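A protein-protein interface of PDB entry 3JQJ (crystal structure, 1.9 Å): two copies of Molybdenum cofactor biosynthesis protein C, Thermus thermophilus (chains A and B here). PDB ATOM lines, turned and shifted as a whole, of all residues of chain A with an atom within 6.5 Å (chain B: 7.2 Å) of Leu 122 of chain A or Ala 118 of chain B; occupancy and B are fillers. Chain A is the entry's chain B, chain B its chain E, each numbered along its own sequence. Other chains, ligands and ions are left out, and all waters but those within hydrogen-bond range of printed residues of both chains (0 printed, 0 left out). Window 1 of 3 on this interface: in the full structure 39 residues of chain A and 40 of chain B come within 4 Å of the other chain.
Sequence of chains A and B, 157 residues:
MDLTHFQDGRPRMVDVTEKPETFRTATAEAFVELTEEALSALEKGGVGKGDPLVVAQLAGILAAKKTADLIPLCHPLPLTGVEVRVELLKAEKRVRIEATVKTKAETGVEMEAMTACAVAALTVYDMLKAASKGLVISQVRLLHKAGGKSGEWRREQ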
ATOM      1  N   VAL A  32     -11.316   2.556  22.826  1.00  0.00           N
ATOM      2  CA  VAL A  32     -10.564   2.611  24.070  1.00  0.00           C
ATOM      3  C   VAL A  32      -9.399   1.666  23.806  1.00  0.00           C
ATOM      4  O   VAL A  32      -9.597   0.474  23.571  1.00  0.00           O
ATOM      5  CB  VAL A  32     -11.375   2.092  25.275  1.00  0.00           C
ATOM      6  CG1 VAL A  32     -10.500   2.103  26.526  1.00  0.00           C
ATOM      7  CG2 VAL A  32     -12.601   2.964  25.491  1.00  0.00           C
ATOM      8  N   ILE A  97     -16.784   1.060  20.366  1.00  0.00           N
ATOM      9  CA  ILE A  97     -18.134   1.414  20.766  1.00  0.00           C
ATOM     10  C   ILE A  97     -18.830   2.098  19.601  1.00  0.00           C
ATOM     11  O   ILE A  97     -18.253   2.963  18.944  1.00  0.00           O
ATOM     12  CB  ILE A  97     -18.137   2.394  21.957  1.00  0.00           C
ATOM     13  CG1 ILE A  97     -17.578   1.711  23.204  1.00  0.00           C
ATOM     14  CG2 ILE A  97     -19.555   2.909  22.199  1.00  0.00           C
ATOM     15  CD1 ILE A  97     -16.348   2.389  23.753  1.00  0.00           C
ATOM     16  N   CYS A 117     -21.306   7.402  22.830  1.00  0.00           N
ATOM     17  CA  CYS A 117     -20.025   6.729  22.626  1.00  0.00           C
ATOM     18  C   CYS A 117     -18.962   7.207  23.611  1.00  0.00           C
ATOM     19  O   CYS A 117     -18.219   6.402  24.173  1.00  0.00           O
ATOM     20  CB  CYS A 117     -19.536   6.932  21.193  1.00  0.00           C
ATOM     21  SG  CYS A 117     -20.501   6.030  19.956  1.00  0.00           S
ATOM     22  N   ALA A 118     -18.897   8.515  23.835  1.00  0.00           N
ATOM     23  CA  ALA A 118     -17.911   9.068  24.757  1.00  0.00           C
ATOM     24  C   ALA A 118     -18.098   8.551  26.181  1.00  0.00           C
ATOM     25  O   ALA A 118     -17.133   8.137  26.825  1.00  0.00           O
ATOM     26  CB  ALA A 118     -17.977  10.596  24.742  1.00  0.00           C
ATOM     27  N   VAL A 119     -19.334   8.562  26.674  1.00  0.00           N
ATOM     28  CA  VAL A 119     -19.587   8.104  28.034  1.00  0.00           C
ATOM     29  C   VAL A 119     -19.394   6.603  28.180  1.00  0.00           C
ATOM     30  O   VAL A 119     -18.952   6.134  29.228  1.00  0.00           O
ATOM     31  CB  VAL A 119     -21.000   8.508  28.513  1.00  0.00           C
ATOM     32  CG1 VAL A 119     -21.274   7.929  29.896  1.00  0.00           C
ATOM     33  CG2 VAL A 119     -21.102  10.029  28.562  1.00  0.00           C
ATOM     34  N   ALA A 120     -19.724   5.846  27.135  1.00  0.00           N
ATOM     35  CA  ALA A 120     -19.529   4.401  27.189  1.00  0.00           C
ATOM     36  C   ALA A 120     -18.021   4.162  27.328  1.00  0.00           C
ATOM     37  O   ALA A 120     -17.583   3.315  28.105  1.00  0.00           O
ATOM     38  CB  ALA A 120     -20.045   3.748  25.910  1.00  0.00           C
ATOM     39  N   ALA A 121     -17.237   4.924  26.571  1.00  0.00           N
ATOM     40  CA  ALA A 121     -15.782   4.804  26.609  1.00  0.00           C
ATOM     41  C   ALA A 121     -15.226   5.174  27.986  1.00  0.00           C
ATOM     42  O   ALA A 121     -14.304   4.531  28.487  1.00  0.00           O
ATOM     43  CB  ALA A 121     -15.157   5.683  25.537  1.00  0.00           C
ATOM     44  N   LEU A 122     -15.786   6.218  28.594  1.00  0.00           N
ATOM     45  CA  LEU A 122     -15.344   6.648  29.914  1.00  0.00           C
ATOM     46  C   LEU A 122     -15.650   5.547  30.915  1.00  0.00           C
ATOM     47  O   LEU A 122     -14.893   5.314  31.858  1.00  0.00           O
ATOM     48  CB  LEU A 122     -16.074   7.933  30.326  1.00  0.00           C
ATOM     49  CG  LEU A 122     -15.636   9.237  29.655  1.00  0.00           C
ATOM     50  CD1 LEU A 122     -16.649  10.336  29.961  1.00  0.00           C
ATOM     51  CD2 LEU A 122     -14.245   9.629  30.162  1.00  0.00           C
ATOM     52  N   THR A 123     -16.763   4.855  30.705  1.00  0.00           N
ATOM     53  CA  THR A 123     -17.138   3.785  31.616  1.00  0.00           C
ATOM     54  C   THR A 123     -16.210   2.591  31.466  1.00  0.00           C
ATOM     55  O   THR A 123     -15.910   1.908  32.445  1.00  0.00           O
ATOM     56  CB  THR A 123     -18.589   3.350  31.385  1.00  0.00           C
ATOM     57  OG1 THR A 123     -19.452   4.469  31.627  1.00  0.00           O
ATOM     58  CG2 THR A 123     -18.964   2.213  32.326  1.00  0.00           C
ATOM     59  N   VAL A 124     -15.764   2.328  30.241  1.00  0.00           N
ATOM     60  CA  VAL A 124     -14.843   1.216  30.020  1.00  0.00           C
ATOM     61  C   VAL A 124     -13.590   1.571  30.808  1.00  0.00           C
ATOM     62  O   VAL A 124     -13.029   0.737  31.522  1.00  0.00           O
ATOM     63  CB  VAL A 124     -14.476   1.056  28.526  1.00  0.00           C
ATOM     64  CG1 VAL A 124     -13.329   0.056  28.375  1.00  0.00           C
ATOM     65  CG2 VAL A 124     -15.696   0.578  27.736  1.00  0.00           C
ATOM     66  N   TYR A 125     -13.161   2.823  30.674  1.00  0.00           N
ATOM     67  CA  TYR A 125     -11.986   3.306  31.390  1.00  0.00           C
ATOM     68  C   TYR A 125     -12.166   3.088  32.892  1.00  0.00           C
ATOM     69  O   TYR A 125     -11.279   2.559  33.565  1.00  0.00           O
ATOM     70  CB  TYR A 125     -11.770   4.795  31.124  1.00  0.00           C
ATOM     71  CG  TYR A 125     -10.576   5.348  31.867  1.00  0.00           C
ATOM     72  CD1 TYR A 125      -9.281   5.130  31.401  1.00  0.00           C
ATOM     73  CD2 TYR A 125     -10.738   6.015  33.079  1.00  0.00           C
ATOM     74  CE1 TYR A 125      -8.170   5.556  32.130  1.00  0.00           C
ATOM     75  CE2 TYR A 125      -9.636   6.446  33.820  1.00  0.00           C
ATOM     76  CZ  TYR A 125      -8.353   6.208  33.338  1.00  0.00           C
ATOM     77  OH  TYR A 125      -7.258   6.594  34.083  1.00  0.00           O
ATOM     78  N   ASP A 126     -13.314   3.502  33.418  1.00  0.00           N
ATOM     79  CA  ASP A 126     -13.597   3.346  34.839  1.00  0.00           C
ATOM     80  C   ASP A 126     -13.560   1.886  35.284  1.00  0.00           C
ATOM     81  O   ASP A 126     -13.109   1.573  36.389  1.00  0.00           O
ATOM     82  CB  ASP A 126     -14.975   3.927  35.179  1.00  0.00           C
ATOM     83  CG  ASP A 126     -15.309   3.801  36.654  1.00  0.00           C
ATOM     84  OD1 ASP A 126     -14.557   4.369  37.469  1.00  0.00           O
ATOM     85  OD2 ASP A 126     -16.314   3.135  37.003  1.00  0.00           O
ATOM     86  N   MET A 127     -14.033   0.997  34.417  1.00  0.00           N
ATOM     87  CA  MET A 127     -14.096  -0.430  34.731  1.00  0.00           C
ATOM     88  C   MET A 127     -12.771  -1.182  34.633  1.00  0.00           C
ATOM     89  O   MET A 127     -12.694  -2.347  35.035  1.00  0.00           O
ATOM     90  CB  MET A 127     -15.117  -1.112  33.817  1.00  0.00           C
ATOM     91  CG  MET A 127     -16.532  -0.557  33.919  1.00  0.00           C
ATOM     92  SD  MET A 127     -17.285  -0.848  35.522  1.00  0.00           S
ATOM     93  CE  MET A 127     -17.524  -2.660  35.448  1.00  0.00           C
ATOM     94  N   ILE A 137      -8.775   6.872  25.564  1.00  0.00           N
ATOM     95  CA  ILE A 137     -10.027   6.900  24.811  1.00  0.00           C
ATOM     96  C   ILE A 137      -9.662   7.600  23.510  1.00  0.00           C
ATOM     97  O   ILE A 137      -9.093   8.690  23.528  1.00  0.00           O
ATOM     98  CB  ILE A 137     -11.131   7.722  25.525  1.00  0.00           C
ATOM     99  CG1 ILE A 137     -11.584   7.002  26.798  1.00  0.00           C
ATOM    100  CG2 ILE A 137     -12.314   7.932  24.577  1.00  0.00           C
ATOM    101  CD1 ILE A 137     -12.582   7.792  27.620  1.00  0.00           C
ATOM    102  N   GLU B  29      -6.457  15.103  30.039  1.00  0.00           N
ATOM    103  CA  GLU B  29      -6.494  16.025  28.912  1.00  0.00           C
ATOM    104  C   GLU B  29      -7.271  15.385  27.772  1.00  0.00           C
ATOM    105  O   GLU B  29      -7.544  14.185  27.793  1.00  0.00           O
ATOM    106  CB  GLU B  29      -5.074  16.381  28.443  1.00  0.00           C
ATOM    107  CG  GLU B  29      -4.373  15.309  27.619  1.00  0.00           C
ATOM    108  CD  GLU B  29      -2.953  15.698  27.211  1.00  0.00           C
ATOM    109  OE1 GLU B  29      -2.587  16.888  27.323  1.00  0.00           O
ATOM    110  OE2 GLU B  29      -2.203  14.806  26.766  1.00  0.00           O
ATOM    111  N   ALA B  30      -7.640  16.194  26.789  1.00  0.00           N
ATOM    112  CA  ALA B  30      -8.374  15.709  25.632  1.00  0.00           C
ATOM    113  C   ALA B  30      -8.086  16.650  24.480  1.00  0.00           C
ATOM    114  O   ALA B  30      -7.698  17.794  24.693  1.00  0.00           O
ATOM    115  CB  ALA B  30      -9.876  15.675  25.926  1.00  0.00           C
ATOM    116  N   VAL B  32      -9.353  17.880  20.301  1.00  0.00           N
ATOM    117  CA  VAL B  32     -10.378  17.896  19.273  1.00  0.00           C
ATOM    118  C   VAL B  32      -9.656  18.313  18.001  1.00  0.00           C
ATOM    119  O   VAL B  32      -9.103  19.409  17.937  1.00  0.00           O
ATOM    120  CB  VAL B  32     -11.479  18.932  19.578  1.00  0.00           C
ATOM    121  CG1 VAL B  32     -12.504  18.935  18.458  1.00  0.00           C
ATOM    122  CG2 VAL B  32     -12.138  18.616  20.912  1.00  0.00           C
ATOM    123  N   GLY B  60     -17.095  21.655  30.821  1.00  0.00           N
ATOM    124  CA  GLY B  60     -16.177  20.751  31.490  1.00  0.00           C
ATOM    125  C   GLY B  60     -16.288  20.838  32.998  1.00  0.00           C
ATOM    126  O   GLY B  60     -16.297  19.820  33.683  1.00  0.00           O
ATOM    127  N   ALA B  63     -19.454  19.230  33.979  1.00  0.00           N
ATOM    128  CA  ALA B  63     -19.372  17.790  33.768  1.00  0.00           C
ATOM    129  C   ALA B  63     -18.620  17.079  34.890  1.00  0.00           C
ATOM    130  O   ALA B  63     -18.950  15.948  35.247  1.00  0.00           O
ATOM    131  CB  ALA B  63     -18.720  17.499  32.422  1.00  0.00           C
ATOM    132  N   LEU B  70     -23.066  10.011  35.514  1.00  0.00           N
ATOM    133  CA  LEU B  70     -22.776   9.488  34.175  1.00  0.00           C
ATOM    134  C   LEU B  70     -22.081   8.126  34.170  1.00  0.00           C
ATOM    135  O   LEU B  70     -22.324   7.300  33.287  1.00  0.00           O
ATOM    136  CB  LEU B  70     -21.909  10.485  33.402  1.00  0.00           C
ATOM    137  CG  LEU B  70     -22.498  11.876  33.168  1.00  0.00           C
ATOM    138  CD1 LEU B  70     -21.447  12.772  32.541  1.00  0.00           C
ATOM    139  CD2 LEU B  70     -23.722  11.770  32.280  1.00  0.00           C
ATOM    140  N   ILE B  71     -21.209   7.907  35.150  1.00  0.00           N
ATOM    141  CA  ILE B  71     -20.461   6.660  35.278  1.00  0.00           C
ATOM    142  C   ILE B  71     -21.153   5.819  36.345  1.00  0.00           C
ATOM    143  O   ILE B  71     -21.070   6.117  37.535  1.00  0.00           O
ATOM    144  CB  ILE B  71     -19.008   6.949  35.695  1.00  0.00           C
ATOM    145  CG1 ILE B  71     -18.468   8.129  34.883  1.00  0.00           C
ATOM    146  CG2 ILE B  71     -18.151   5.714  35.504  1.00  0.00           C
ATOM    147  CD1 ILE B  71     -18.554   7.956  33.368  1.00  0.00           C
ATOM    148  N   ILE B  97      -7.821  20.377  25.872  1.00  0.00           N
ATOM    149  CA  ILE B  97      -8.540  20.564  27.117  1.00  0.00           C
ATOM    150  C   ILE B  97      -7.795  19.830  28.220  1.00  0.00           C
ATOM    151  O   ILE B  97      -7.342  18.698  28.034  1.00  0.00           O
ATOM    152  CB  ILE B  97      -9.966  19.981  27.043  1.00  0.00           C
ATOM    153  CG1 ILE B  97     -10.703  20.556  25.837  1.00  0.00           C
ATOM    154  CG2 ILE B  97     -10.725  20.304  28.329  1.00  0.00           C
ATOM    155  CD1 ILE B  97     -11.433  19.513  25.029  1.00  0.00           C
ATOM    156  N   GLU B 110     -10.049  10.261  39.287  1.00  0.00           N
ATOM    157  CA  GLU B 110      -9.605  10.142  37.905  1.00  0.00           C
ATOM    158  C   GLU B 110     -10.785  10.330  36.949  1.00  0.00           C
ATOM    159  O   GLU B 110     -10.665  11.016  35.935  1.00  0.00           O
ATOM    160  CB  GLU B 110      -8.962   8.770  37.653  1.00  0.00           C
ATOM    161  CG  GLU B 110      -7.661   8.544  38.404  1.00  0.00           C
ATOM    162  CD  GLU B 110      -7.870   7.932  39.777  1.00  0.00           C
ATOM    163  OE1 GLU B 110      -8.988   8.059  40.329  1.00  0.00           O
ATOM    164  OE2 GLU B 110      -6.909   7.331  40.305  1.00  0.00           O
ATOM    165  N   MET B 111     -11.925   9.727  37.279  1.00  0.00           N
ATOM    166  CA  MET B 111     -13.107   9.835  36.415  1.00  0.00           C
ATOM    167  C   MET B 111     -13.587  11.266  36.226  1.00  0.00           C
ATOM    168  O   MET B 111     -13.886  11.677  35.104  1.00  0.00           O
ATOM    169  CB  MET B 111     -14.254   8.980  36.961  1.00  0.00           C
ATOM    170  CG  MET B 111     -14.002   7.484  36.868  1.00  0.00           C
ATOM    171  SD  MET B 111     -13.290   7.030  35.256  1.00  0.00           S
ATOM    172  CE  MET B 111     -14.572   7.578  34.144  1.00  0.00           C
ATOM    173  N   GLU B 112     -13.662  12.024  37.315  1.00  0.00           N
ATOM    174  CA  GLU B 112     -14.111  13.407  37.234  1.00  0.00           C
ATOM    175  C   GLU B 112     -13.265  14.205  36.249  1.00  0.00           C
ATOM    176  O   GLU B 112     -13.788  15.017  35.493  1.00  0.00           O
ATOM    177  CB  GLU B 112     -14.059  14.083  38.611  1.00  0.00           C
ATOM    178  CG  GLU B 112     -15.156  13.665  39.596  1.00  0.00           C
ATOM    179  CD  GLU B 112     -14.957  12.278  40.169  1.00  0.00           C
ATOM    180  OE1 GLU B 112     -13.865  11.701  39.993  1.00  0.00           O
ATOM    181  OE2 GLU B 112     -15.895  11.763  40.816  1.00  0.00           O
ATOM    182  N   ALA B 113     -11.954  13.979  36.263  1.00  0.00           N
ATOM    183  CA  ALA B 113     -11.052  14.696  35.361  1.00  0.00           C
ATOM    184  C   ALA B 113     -11.240  14.238  33.920  1.00  0.00           C
ATOM    185  O   ALA B 113     -11.252  15.057  32.988  1.00  0.00           O
ATOM    186  CB  ALA B 113      -9.601  14.485  35.790  1.00  0.00           C
ATOM    187  N   MET B 114     -11.370  12.926  33.743  1.00  0.00           N
ATOM    188  CA  MET B 114     -11.571  12.352  32.418  1.00  0.00           C
ATOM    189  C   MET B 114     -12.891  12.839  31.814  1.00  0.00           C
ATOM    190  O   MET B 114     -12.947  13.239  30.646  1.00  0.00           O
ATOM    191  CB  MET B 114     -11.583  10.824  32.507  1.00  0.00           C
ATOM    192  CG  MET B 114     -10.225  10.187  32.807  1.00  0.00           C
ATOM    193  SD  MET B 114      -9.075  10.338  31.426  1.00  0.00           S
ATOM    194  CE  MET B 114      -9.696   9.027  30.340  1.00  0.00           C
ATOM    195  N   THR B 115     -13.945  12.794  32.620  1.00  0.00           N
ATOM    196  CA  THR B 115     -15.274  13.215  32.181  1.00  0.00           C
ATOM    197  C   THR B 115     -15.305  14.704  31.842  1.00  0.00           C
ATOM    198  O   THR B 115     -15.892  15.109  30.838  1.00  0.00           O
ATOM    199  CB  THR B 115     -16.318  12.915  33.266  1.00  0.00           C
ATOM    200  OG1 THR B 115     -16.338  11.505  33.522  1.00  0.00           O
ATOM    201  CG2 THR B 115     -17.709  13.375  32.822  1.00  0.00           C
ATOM    202  N   ALA B 116     -14.673  15.521  32.678  1.00  0.00           N
ATOM    203  CA  ALA B 116     -14.637  16.959  32.426  1.00  0.00           C
ATOM    204  C   ALA B 116     -14.037  17.242  31.049  1.00  0.00           C
ATOM    205  O   ALA B 116     -14.552  18.068  30.290  1.00  0.00           O
ATOM    206  CB  ALA B 116     -13.822  17.666  33.516  1.00  0.00           C
ATOM    207  N   CYS B 117     -12.948  16.551  30.722  1.00  0.00           N
ATOM    208  CA  CYS B 117     -12.294  16.743  29.432  1.00  0.00           C
ATOM    209  C   CYS B 117     -13.136  16.228  28.272  1.00  0.00           C
ATOM    210  O   CYS B 117     -13.239  16.875  27.232  1.00  0.00           O
ATOM    211  CB  CYS B 117     -10.932  16.044  29.417  1.00  0.00           C
ATOM    212  SG  CYS B 117      -9.704  16.803  30.506  1.00  0.00           S
ATOM    213  N   ALA B 118     -13.728  15.053  28.449  1.00  0.00           N
ATOM    214  CA  ALA B 118     -14.549  14.457  27.399  1.00  0.00           C
ATOM    215  C   ALA B 118     -15.753  15.327  27.050  1.00  0.00           C
ATOM    216  O   ALA B 118     -16.024  15.585  25.879  1.00  0.00           O
ATOM    217  CB  ALA B 118     -15.014  13.074  27.828  1.00  0.00           C
ATOM    218  N   VAL B 119     -16.475  15.785  28.065  1.00  0.00           N
ATOM    219  CA  VAL B 119     -17.654  16.600  27.806  1.00  0.00           C
ATOM    220  C   VAL B 119     -17.275  17.947  27.208  1.00  0.00           C
ATOM    221  O   VAL B 119     -17.975  18.467  26.340  1.00  0.00           O
ATOM    222  CB  VAL B 119     -18.476  16.807  29.085  1.00  0.00           C
ATOM    223  CG1 VAL B 119     -19.667  17.725  28.797  1.00  0.00           C
ATOM    224  CG2 VAL B 119     -18.965  15.460  29.603  1.00  0.00           C
ATOM    225  N   ALA B 120     -16.165  18.510  27.669  1.00  0.00           N
ATOM    226  CA  ALA B 120     -15.708  19.782  27.133  1.00  0.00           C
ATOM    227  C   ALA B 120     -15.443  19.586  25.640  1.00  0.00           C
ATOM    228  O   ALA B 120     -15.774  20.441  24.819  1.00  0.00           O
ATOM    229  CB  ALA B 120     -14.432  20.231  27.852  1.00  0.00           C
ATOM    230  N   ALA B 121     -14.851  18.443  25.296  1.00  0.00           N
ATOM    231  CA  ALA B 121     -14.545  18.118  23.905  1.00  0.00           C
ATOM    232  C   ALA B 121     -15.838  17.952  23.104  1.00  0.00           C
ATOM    233  O   ALA B 121     -15.945  18.432  21.976  1.00  0.00           O
ATOM    234  CB  ALA B 121     -13.711  16.834  23.837  1.00  0.00           C
ATOM    235  N   LEU B 122     -16.812  17.255  23.684  1.00  0.00           N
ATOM    236  CA  LEU B 122     -18.103  17.062  23.022  1.00  0.00           C
ATOM    237  C   LEU B 122     -18.751  18.424  22.781  1.00  0.00           C
ATOM    238  O   LEU B 122     -19.387  18.651  21.750  1.00  0.00           O
ATOM    239  CB  LEU B 122     -19.032  16.208  23.892  1.00  0.00           C
ATOM    240  CG  LEU B 122     -18.723  14.712  24.009  1.00  0.00           C
ATOM    241  CD1 LEU B 122     -19.543  14.116  25.141  1.00  0.00           C
ATOM    242  CD2 LEU B 122     -19.030  14.017  22.681  1.00  0.00           C
ATOM    243  N   THR B 123     -18.584  19.340  23.729  1.00  0.00           N
ATOM    244  CA  THR B 123     -19.183  20.657  23.568  1.00  0.00           C
ATOM    245  C   THR B 123     -18.485  21.426  22.449  1.00  0.00           C
ATOM    246  O   THR B 123     -19.128  22.144  21.690  1.00  0.00           O
ATOM    247  CB  THR B 123     -19.151  21.453  24.888  1.00  0.00           C
ATOM    248  OG1 THR B 123     -19.905  20.741  25.883  1.00  0.00           O
ATOM    249  CG2 THR B 123     -19.765  22.839  24.690  1.00  0.00           C
ATOM    250  N   VAL B 124     -17.170  21.270  22.330  1.00  0.00           N
ATOM    251  CA  VAL B 124     -16.450  21.944  21.256  1.00  0.00           C
ATOM    252  C   VAL B 124     -17.023  21.438  19.930  1.00  0.00           C
ATOM    253  O   VAL B 124     -17.251  22.205  18.996  1.00  0.00           O
ATOM    254  CB  VAL B 124     -14.931  21.636  21.319  1.00  0.00           C
ATOM    255  CG1 VAL B 124     -14.234  22.168  20.077  1.00  0.00           C
ATOM    256  CG2 VAL B 124     -14.329  22.261  22.573  1.00  0.00           C
ATOM    257  N   ILE B 137     -12.749  13.797  18.180  1.00  0.00           N
ATOM    258  CA  ILE B 137     -12.196  13.936  19.521  1.00  0.00           C
ATOM    259  C   ILE B 137     -11.146  12.825  19.485  1.00  0.00           C
ATOM    260  O   ILE B 137     -11.451  11.660  19.729  1.00  0.00           O
ATOM    261  CB  ILE B 137     -13.248  13.640  20.610  1.00  0.00           C
ATOM    262  CG1 ILE B 137     -14.389  14.661  20.518  1.00  0.00           C
ATOM    263  CG2 ILE B 137     -12.600  13.682  21.989  1.00  0.00           C
ATOM    264  CD1 ILE B 137     -15.563  14.377  21.448  1.00  0.00           C
ATOM    265  N   GLN B 139      -8.286  12.054  21.378  1.00  0.00           N
ATOM    266  CA  GLN B 139      -7.937  11.338  22.596  1.00  0.00           C
ATOM    267  C   GLN B 139      -8.451  11.991  23.871  1.00  0.00           C
ATOM    268  O   GLN B 139      -8.778  13.176  23.901  1.00  0.00           O
ATOM    269  CB  GLN B 139      -6.415  11.197  22.718  1.00  0.00           C
ATOM    270  CG  GLN B 139      -5.718  10.684  21.469  1.00  0.00           C
ATOM    271  CD  GLN B 139      -4.269  10.291  21.711  1.00  0.00           C
ATOM    272  OE1 GLN B 139      -3.502  10.117  20.767  1.00  0.00           O
ATOM    273  NE2 GLN B 139      -3.892  10.134  22.976  1.00  0.00           N
ATOM    274  N   VAL B 140      -8.513  11.181  24.919  1.00  0.00           N
ATOM    275  CA  VAL B 140      -8.915  11.601  26.253  1.00  0.00           C
ATOM    276  C   VAL B 140      -8.058  10.667  27.099  1.00  0.00           C
ATOM    277  O   VAL B 140      -8.216   9.449  27.038  1.00  0.00           O
ATOM    278  CB  VAL B 140     -10.412  11.335  26.532  1.00  0.00           C
ATOM    279  CG1 VAL B 140     -10.784  11.887  27.909  1.00  0.00           C
ATOM    280  CG2 VAL B 140     -11.269  11.987  25.461  1.00  0.00           C
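Printed residues of chain B within 4 Å of Leu 122 of chain A: Ile 71, Met 111, Met 114, Thr 115 and Ala 118.
Of chain A, only Leu 122 comes within 4 Å of Ala 118 of chain B.
Of the printed residues of chain A, Leu 122 of chain B touches Ala 118.
Printed residues of chain B within 4 Å of Ile 137 of chain A: Gln 139 and Val 140.
The nearest residue of chain B that does not touch Leu 122 of chain A is Val 140 of chain B (4.7 Å).
The nearest printed residue of chain B that does not touch Ala 118 of chain A is Ala 118 of chain B (4.9 Å).
Ala 118 of chain A touches Leu 122 of chain B, and with the chains exchanged Leu 122 of chain A touches Ala 118 of chain B.
Positions printed for both chains: 32, 97, 117, 118, 119, 120, 121, 122, 123, 124 and 137.
Of the 14 pairs that touch across the chains among the printed residues, 2 have their exchanged pair printed and touching as well.
The side-chain hydroxyl (OG1) of Thr 123 of chain A is in hydrogen-bond range of the backbone carbonyl oxygen (O) of Val 119 of chain A (3.0 Å).
O of Met 111 of chain B is in hydrogen-bond range of OG1 of Thr 115 of chain B (2.9 Å).
Among the printed residues, merely in contact across the chains: Ile 137 of chain A with Gln 139 of chain B (3.0 Å), Leu 122 of chain A with Met 111 of chain B (3.2 Å), Asp 126 of chain A with Ile 71 of chain B (3.5 Å), Tyr 125 of chain A with Met 111 of chain B (3.5 Å), Val 119 of chain A with Leu 70 of chain B (3.6 Å), Leu 122 of chain A with Met 114 of chain B (3.7 Å), Leu 122 of chain A with Thr 115 of chain B (3.8 Å), Leu 122 of chain A with Ala 118 of chain B (3.8 Å), Ala 118 of chain A with Leu 122 of chain B (3.9 Å), Tyr 125 of chain A with Met 114 of chain B (3.9 Å), Leu 122 of chain A with Ile 71 of chain B (3.9 Å) and Thr 123 of chain A with Ile 71 of chain B (3.9996 Å).
Hydrophobic or aromatic side chains of chain B that line the printed part of chain A: Ile 71, Met 111, Met 114, Ala 118, Leu 122 and Val 140.
Printed residues of chain A that touch a printed residue of chain B: Ala 118, Val 119, Leu 122, Thr 123, Tyr 125, Asp 126 and Ile 137.
Hydrophobic or aromatic side chains of chain A within 4 Å of the printed part of chain B: Ala 118, Val 119, Leu 122, Tyr 125 and Ile 137.
Among the printed residues, 14 pairs touch across the chains.
Among the printed residues, no Asp or Glu carboxylate lies within 4 Å of a Lys or Arg side-chain nitrogen of the other chain.
The backbone carbonyl oxygen (O) of Ile 137 of chain A sits at hydrogen-bond distance from the backbone NH (N) of Val 140 of chain B (2.9 Å).
The side-chain carboxylate of Asp 126 of chain A sits close to the side-chain sulfur of Met 111 of chain B (3.7 Å).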
